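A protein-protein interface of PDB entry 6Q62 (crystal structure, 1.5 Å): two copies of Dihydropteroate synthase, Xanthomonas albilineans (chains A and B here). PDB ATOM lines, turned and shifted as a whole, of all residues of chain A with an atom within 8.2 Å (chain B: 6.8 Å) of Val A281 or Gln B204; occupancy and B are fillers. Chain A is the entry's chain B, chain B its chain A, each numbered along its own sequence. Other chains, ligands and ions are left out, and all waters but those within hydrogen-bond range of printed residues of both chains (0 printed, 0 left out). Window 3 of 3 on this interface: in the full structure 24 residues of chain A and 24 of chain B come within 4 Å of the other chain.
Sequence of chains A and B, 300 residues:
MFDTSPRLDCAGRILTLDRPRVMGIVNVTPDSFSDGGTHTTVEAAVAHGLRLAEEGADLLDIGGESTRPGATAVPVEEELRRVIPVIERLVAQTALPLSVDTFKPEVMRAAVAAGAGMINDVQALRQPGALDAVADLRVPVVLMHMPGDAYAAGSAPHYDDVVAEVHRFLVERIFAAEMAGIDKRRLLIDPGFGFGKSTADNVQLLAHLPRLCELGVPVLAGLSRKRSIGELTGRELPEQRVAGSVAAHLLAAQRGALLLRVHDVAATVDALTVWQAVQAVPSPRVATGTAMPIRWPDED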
ATOM      1  N   TRP A 275      -0.470   2.999  24.416  1.00  0.00           N
ATOM      2  CA  TRP A 275       0.485   3.547  23.459  1.00  0.00           C
ATOM      3  C   TRP A 275       0.080   3.271  22.013  1.00  0.00           C
ATOM      4  O   TRP A 275       0.122   4.211  21.203  1.00  0.00           O
ATOM      5  CB  TRP A 275       1.898   3.029  23.746  1.00  0.00           C
ATOM      6  CG  TRP A 275       2.906   3.390  22.696  1.00  0.00           C
ATOM      7  CD1 TRP A 275       3.283   4.641  22.298  1.00  0.00           C
ATOM      8  CD2 TRP A 275       3.652   2.472  21.907  1.00  0.00           C
ATOM      9  NE1 TRP A 275       4.215   4.554  21.294  1.00  0.00           N
ATOM     10  CE2 TRP A 275       4.481   3.232  21.050  1.00  0.00           C
ATOM     11  CE3 TRP A 275       3.704   1.072  21.838  1.00  0.00           C
ATOM     12  CZ2 TRP A 275       5.354   2.637  20.138  1.00  0.00           C
ATOM     13  CZ3 TRP A 275       4.576   0.480  20.933  1.00  0.00           C
ATOM     14  CH2 TRP A 275       5.391   1.261  20.101  1.00  0.00           C
ATOM     15  N   GLN A 276      -0.340   2.019  21.694  1.00  0.00           N
ATOM     16  CA  GLN A 276      -0.777   1.662  20.336  1.00  0.00           C
ATOM     17  C   GLN A 276      -1.939   2.539  19.868  1.00  0.00           C
ATOM     18  O   GLN A 276      -1.927   2.982  18.719  1.00  0.00           O
ATOM     19  CB  GLN A 276      -1.159   0.177  20.233  1.00  0.00           C
ATOM     20  CG  GLN A 276       0.058  -0.767  20.088  1.00  0.00           C
ATOM     21  CD  GLN A 276       0.769  -0.659  18.766  1.00  0.00           C
ATOM     22  OE1 GLN A 276       0.195  -0.890  17.693  1.00  0.00           O
ATOM     23  NE2 GLN A 276       2.042  -0.322  18.819  1.00  0.00           N
ATOM     24  N   ALA A 277      -2.912   2.829  20.754  1.00  0.00           N
ATOM     25  CA  ALA A 277      -4.068   3.675  20.424  1.00  0.00           C
ATOM     26  C   ALA A 277      -3.629   5.087  20.067  1.00  0.00           C
ATOM     27  O   ALA A 277      -4.101   5.642  19.087  1.00  0.00           O
ATOM     28  CB  ALA A 277      -5.044   3.711  21.593  1.00  0.00           C
ATOM     29  N   VAL A 278      -2.687   5.643  20.838  1.00  0.00           N
ATOM     30  CA  VAL A 278      -2.150   6.974  20.643  1.00  0.00           C
ATOM     31  C   VAL A 278      -1.307   7.051  19.365  1.00  0.00           C
ATOM     32  O   VAL A 278      -1.494   7.977  18.572  1.00  0.00           O
ATOM     33  CB  VAL A 278      -1.369   7.435  21.902  1.00  0.00           C
ATOM     34  CG1 VAL A 278      -0.605   8.720  21.651  1.00  0.00           C
ATOM     35  CG2 VAL A 278      -2.309   7.596  23.093  1.00  0.00           C
ATOM     36  N   GLN A 279      -0.386   6.087  19.173  1.00  0.00           N
ATOM     37  CA  GLN A 279       0.519   6.016  18.022  1.00  0.00           C
ATOM     38  C   GLN A 279      -0.268   5.875  16.700  1.00  0.00           C
ATOM     39  O   GLN A 279       0.210   6.332  15.660  1.00  0.00           O
ATOM     40  CB  GLN A 279       1.498   4.837  18.206  1.00  0.00           C
ATOM     41  CG  GLN A 279       2.915   5.117  17.722  1.00  0.00           C
ATOM     42  CD  GLN A 279       3.610   3.895  17.151  1.00  0.00           C
ATOM     43  OE1 GLN A 279       3.018   2.827  16.944  1.00  0.00           O
ATOM     44  NE2 GLN A 279       4.892   4.036  16.866  1.00  0.00           N
ATOM     45  N   ALA A 280      -1.464   5.262  16.749  1.00  0.00           N
ATOM     46  CA  ALA A 280      -2.348   5.035  15.597  1.00  0.00           C
ATOM     47  C   ALA A 280      -2.976   6.310  15.045  1.00  0.00           C
ATOM     48  O   ALA A 280      -3.537   6.280  13.952  1.00  0.00           O
ATOM     49  CB  ALA A 280      -3.435   4.045  15.958  1.00  0.00           C
ATOM     50  N   VAL A 281      -2.923   7.417  15.804  1.00  0.00           N
ATOM     51  CA  VAL A 281      -3.533   8.677  15.379  1.00  0.00           C
ATOM     52  C   VAL A 281      -2.631   9.393  14.373  1.00  0.00           C
ATOM     53  O   VAL A 281      -1.487   9.717  14.711  1.00  0.00           O
ATOM     54  CB  VAL A 281      -3.958   9.585  16.579  1.00  0.00           C
ATOM     55  CG1 VAL A 281      -4.476  10.943  16.104  1.00  0.00           C
ATOM     56  CG2 VAL A 281      -5.013   8.905  17.439  1.00  0.00           C
ATOM     57  N   PRO A 282      -3.151   9.678  13.145  1.00  0.00           N
ATOM     58  CA  PRO A 282      -2.336  10.408  12.158  1.00  0.00           C
ATOM     59  C   PRO A 282      -2.242  11.901  12.473  1.00  0.00           C
ATOM     60  O   PRO A 282      -1.342  12.342  13.183  1.00  0.00           O
ATOM     61  CB  PRO A 282      -3.073  10.155  10.841  1.00  0.00           C
ATOM     62  CG  PRO A 282      -4.493   9.940  11.230  1.00  0.00           C
ATOM     63  CD  PRO A 282      -4.496   9.360  12.616  1.00  0.00           C
ATOM     64  N   ASP B 161     -14.203  19.034  15.276  1.00  0.00           N
ATOM     65  CA  ASP B 161     -12.762  18.909  15.446  1.00  0.00           C
ATOM     66  C   ASP B 161     -12.466  19.174  16.929  1.00  0.00           C
ATOM     67  O   ASP B 161     -12.265  20.327  17.323  1.00  0.00           O
ATOM     68  CB  ASP B 161     -12.055  19.939  14.534  1.00  0.00           C
ATOM     69  CG  ASP B 161     -10.544  19.835  14.397  1.00  0.00           C
ATOM     70  OD1 ASP B 161      -9.899  19.215  15.279  1.00  0.00           O
ATOM     71  OD2 ASP B 161      -9.998  20.414  13.435  1.00  0.00           O
ATOM     72  N   VAL B 162     -12.459  18.111  17.752  1.00  0.00           N
ATOM     73  CA  VAL B 162     -12.234  18.227  19.205  1.00  0.00           C
ATOM     74  C   VAL B 162     -10.928  18.979  19.559  1.00  0.00           C
ATOM     75  O   VAL B 162     -10.943  19.795  20.469  1.00  0.00           O
ATOM     76  CB  VAL B 162     -12.343  16.863  19.948  1.00  0.00           C
ATOM     77  CG1 VAL B 162     -11.131  15.954  19.683  1.00  0.00           C
ATOM     78  CG2 VAL B 162     -12.546  17.074  21.451  1.00  0.00           C
ATOM     79  N   VAL B 163      -9.824  18.733  18.838  1.00  0.00           N
ATOM     80  CA  VAL B 163      -8.532  19.380  19.124  1.00  0.00           C
ATOM     81  C   VAL B 163      -8.618  20.884  18.891  1.00  0.00           C
ATOM     82  O   VAL B 163      -8.140  21.677  19.721  1.00  0.00           O
ATOM     83  CB  VAL B 163      -7.373  18.728  18.299  1.00  0.00           C
ATOM     84  CG1 VAL B 163      -6.067  19.533  18.409  1.00  0.00           C
ATOM     85  CG2 VAL B 163      -7.148  17.296  18.742  1.00  0.00           C
ATOM     86  N   PHE B 193      -9.500  15.827  29.954  1.00  0.00           N
ATOM     87  CA  PHE B 193      -9.780  14.463  29.498  1.00  0.00           C
ATOM     88  C   PHE B 193     -10.980  13.874  30.248  1.00  0.00           C
ATOM     89  O   PHE B 193     -11.083  14.012  31.469  1.00  0.00           O
ATOM     90  CB  PHE B 193      -8.543  13.571  29.688  1.00  0.00           C
ATOM     91  CG  PHE B 193      -7.398  13.939  28.780  1.00  0.00           C
ATOM     92  CD1 PHE B 193      -7.422  13.603  27.438  1.00  0.00           C
ATOM     93  CD2 PHE B 193      -6.239  14.525  29.293  1.00  0.00           C
ATOM     94  CE1 PHE B 193      -6.344  13.924  26.595  1.00  0.00           C
ATOM     95  CE2 PHE B 193      -5.151  14.819  28.453  1.00  0.00           C
ATOM     96  CZ  PHE B 193      -5.209  14.518  27.111  1.00  0.00           C
ATOM     97  N   THR B 199     -13.921   8.190  24.152  1.00  0.00           N
ATOM     98  CA  THR B 199     -12.561   7.624  24.183  1.00  0.00           C
ATOM     99  C   THR B 199     -11.775   8.128  22.964  1.00  0.00           C
ATOM    100  O   THR B 199     -10.649   8.591  23.133  1.00  0.00           O
ATOM    101  CB  THR B 199     -12.600   6.086  24.295  1.00  0.00           C
ATOM    102  OG1 THR B 199     -13.293   5.755  25.489  1.00  0.00           O
ATOM    103  CG2 THR B 199     -11.211   5.448  24.336  1.00  0.00           C
ATOM    104  N   ALA B 200     -12.390   8.106  21.750  1.00  0.00           N
ATOM    105  CA  ALA B 200     -11.746   8.582  20.525  1.00  0.00           C
ATOM    106  C   ALA B 200     -11.302  10.045  20.671  1.00  0.00           C
ATOM    107  O   ALA B 200     -10.199  10.389  20.232  1.00  0.00           O
ATOM    108  CB  ALA B 200     -12.692   8.425  19.321  1.00  0.00           C
ATOM    109  N   ASP B 201     -12.162  10.912  21.272  1.00  0.00           N
ATOM    110  CA  ASP B 201     -11.820  12.331  21.494  1.00  0.00           C
ATOM    111  C   ASP B 201     -10.648  12.440  22.449  1.00  0.00           C
ATOM    112  O   ASP B 201      -9.781  13.282  22.248  1.00  0.00           O
ATOM    113  CB  ASP B 201     -12.988  13.102  22.118  1.00  0.00           C
ATOM    114  CG  ASP B 201     -14.224  13.255  21.260  1.00  0.00           C
ATOM    115  OD1 ASP B 201     -14.079  13.338  20.017  1.00  0.00           O
ATOM    116  OD2 ASP B 201     -15.338  13.336  21.838  1.00  0.00           O
ATOM    117  N   ASN B 202     -10.648  11.641  23.517  1.00  0.00           N
ATOM    118  CA  ASN B 202      -9.556  11.683  24.508  1.00  0.00           C
ATOM    119  C   ASN B 202      -8.222  11.247  23.885  1.00  0.00           C
ATOM    120  O   ASN B 202      -7.180  11.860  24.138  1.00  0.00           O
ATOM    121  CB  ASN B 202      -9.906  10.810  25.694  1.00  0.00           C
ATOM    122  CG  ASN B 202     -10.936  11.462  26.578  1.00  0.00           C
ATOM    123  OD1 ASN B 202     -10.878  12.653  26.844  1.00  0.00           O
ATOM    124  ND2 ASN B 202     -11.917  10.714  27.021  1.00  0.00           N
ATOM    125  N   VAL B 203      -8.262  10.205  23.033  1.00  0.00           N
ATOM    126  CA  VAL B 203      -7.069   9.705  22.345  1.00  0.00           C
ATOM    127  C   VAL B 203      -6.549  10.770  21.367  1.00  0.00           C
ATOM    128  O   VAL B 203      -5.342  11.026  21.324  1.00  0.00           O
ATOM    129  CB  VAL B 203      -7.356   8.347  21.658  1.00  0.00           C
ATOM    130  CG1 VAL B 203      -6.188   7.912  20.769  1.00  0.00           C
ATOM    131  CG2 VAL B 203      -7.666   7.272  22.694  1.00  0.00           C
ATOM    132  N   GLN B 204      -7.467  11.440  20.630  1.00  0.00           N
ATOM    133  CA  GLN B 204      -7.104  12.528  19.713  1.00  0.00           C
ATOM    134  C   GLN B 204      -6.409  13.660  20.462  1.00  0.00           C
ATOM    135  O   GLN B 204      -5.375  14.152  20.013  1.00  0.00           O
ATOM    136  CB  GLN B 204      -8.339  13.090  18.995  1.00  0.00           C
ATOM    137  CG  GLN B 204      -8.903  12.208  17.874  1.00  0.00           C
ATOM    138  CD  GLN B 204      -8.010  12.124  16.656  1.00  0.00           C
ATOM    139  OE1 GLN B 204      -7.374  13.100  16.232  1.00  0.00           O
ATOM    140  NE2 GLN B 204      -7.957  10.945  16.067  1.00  0.00           N
ATOM    141  N   LEU B 205      -6.975  14.083  21.599  1.00  0.00           N
ATOM    142  CA  LEU B 205      -6.394  15.177  22.380  1.00  0.00           C
ATOM    143  C   LEU B 205      -5.040  14.839  22.939  1.00  0.00           C
ATOM    144  O   LEU B 205      -4.184  15.727  23.034  1.00  0.00           O
ATOM    145  CB  LEU B 205      -7.332  15.592  23.527  1.00  0.00           C
ATOM    146  CG  LEU B 205      -8.582  16.383  23.112  1.00  0.00           C
ATOM    147  CD1 LEU B 205      -9.608  16.334  24.204  1.00  0.00           C
ATOM    148  CD2 LEU B 205      -8.229  17.841  22.762  1.00  0.00           C
ATOM    149  N   LEU B 206      -4.843  13.566  23.343  1.00  0.00           N
ATOM    150  CA  LEU B 206      -3.554  13.115  23.873  1.00  0.00           C
ATOM    151  C   LEU B 206      -2.526  13.029  22.749  1.00  0.00           C
ATOM    152  O   LEU B 206      -1.418  13.533  22.894  1.00  0.00           O
ATOM    153  CB  LEU B 206      -3.695  11.751  24.571  1.00  0.00           C
ATOM    154  CG  LEU B 206      -2.437  11.120  25.198  1.00  0.00           C
ATOM    155  CD1 LEU B 206      -1.721  12.098  26.112  1.00  0.00           C
ATOM    156  CD2 LEU B 206      -2.832   9.869  26.008  1.00  0.00           C
ATOM    157  N   ALA B 207      -2.922  12.470  21.604  1.00  0.00           N
ATOM    158  CA  ALA B 207      -2.005  12.361  20.469  1.00  0.00           C
ATOM    159  C   ALA B 207      -1.575  13.757  19.980  1.00  0.00           C
ATOM    160  O   ALA B 207      -0.408  13.946  19.653  1.00  0.00           O
ATOM    161  CB  ALA B 207      -2.670  11.585  19.338  1.00  0.00           C
ATOM    162  N   HIS B 208      -2.502  14.732  19.991  1.00  0.00           N
ATOM    163  CA  HIS B 208      -2.253  16.108  19.538  1.00  0.00           C
ATOM    164  C   HIS B 208      -1.943  17.093  20.661  1.00  0.00           C
ATOM    165  O   HIS B 208      -1.968  18.304  20.441  1.00  0.00           O
ATOM    166  CB  HIS B 208      -3.414  16.613  18.682  1.00  0.00           C
ATOM    167  CG  HIS B 208      -3.578  15.869  17.403  1.00  0.00           C
ATOM    168  ND1 HIS B 208      -4.555  14.927  17.254  1.00  0.00           N
ATOM    169  CD2 HIS B 208      -2.879  15.962  16.250  1.00  0.00           C
ATOM    170  CE1 HIS B 208      -4.462  14.502  16.007  1.00  0.00           C
ATOM    171  NE2 HIS B 208      -3.447  15.071  15.377  1.00  0.00           N
ATOM    172  N   LEU B 209      -1.589  16.580  21.854  1.00  0.00           N
ATOM    173  CA  LEU B 209      -1.232  17.424  22.995  1.00  0.00           C
ATOM    174  C   LEU B 209      -0.123  18.456  22.687  1.00  0.00           C
ATOM    175  O   LEU B 209      -0.211  19.575  23.204  1.00  0.00           O
ATOM    176  CB  LEU B 209      -0.874  16.568  24.216  1.00  0.00           C
ATOM    177  CG  LEU B 209      -1.067  17.234  25.586  1.00  0.00           C
ATOM    178  CD1 LEU B 209      -2.543  17.569  25.844  1.00  0.00           C
ATOM    179  CD2 LEU B 209      -0.571  16.330  26.692  1.00  0.00           C
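The backbone carbonyl oxygen (O) of Gln B204 lies within hydrogen-bond range of a ring nitrogen (ND1) of His B208, at 3.0 Å.
Of chain B, only Val B203 (3.7 Å), Gln B204 (3.5 Å), Ala B207 (3.6 Å) and His B208 (3.6 Å) come within 4 Å of Val A281.
Of chain A, only Val A281 comes within 4 Å of Gln B204.
Printed residues of chain A within 4 Å of His B208: Val A281 (3.6 Å).
Of the printed residues of chain B, Val A278 touches Leu B206 and Ala B207.
Of the printed residues of chain A, Leu B206 touches Val A278.
Of the printed residues of chain B, Ala A277 touches Val B203.
Leu B205 touches none of the printed residues of chain A.
Asn B202 touches none of the printed residues of chain A.
The nearest residue of chain B that does not touch Val A281 is Ala B200 (6.1 Å).
The nearest printed residue of chain A that does not touch Leu B206 is Val A281 (7.2 Å).
Of the 8 printed residues of chain A, 3 touch a printed residue of chain B.
Hydrophobic or aromatic side chains of chain A within 4 Å of the printed part of chain B: Val A278 and Val A281.
Along chain A the printed residues that touch a printed residue of chain B span positions 277 to 281.
Printed residues of chain B that touch a printed residue of chain A: Val B203, Gln B204, Leu B206, Ala B207 and His B208.
Hydrophobic or aromatic side chains of chain B within 4 Å of the printed part of chain A: Val B203, Leu B206, Ala B207 and His B208.
Among the printed residues, no Asp or Glu carboxylate lies within 4 Å of a Lys or Arg side-chain nitrogen of the other chain.
No position is printed for both chains.
Of the 7 pairs that touch across the chains among the printed residues, none has its exchanged pair printed and touching as well.
Among the printed residues, pairs that only touch across the chains: Val A281 with Gln B204 (3.5 Å), Ala A277 with Val B203 (3.5 Å), Val A281 with His B208 (3.6 Å), Val A281 with Ala B207 (3.6 Å), Val A281 with Val B203 (3.7 Å), Val A278 with Leu B206 (3.7 Å) and Val A278 with Ala B207 (3.9 Å).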
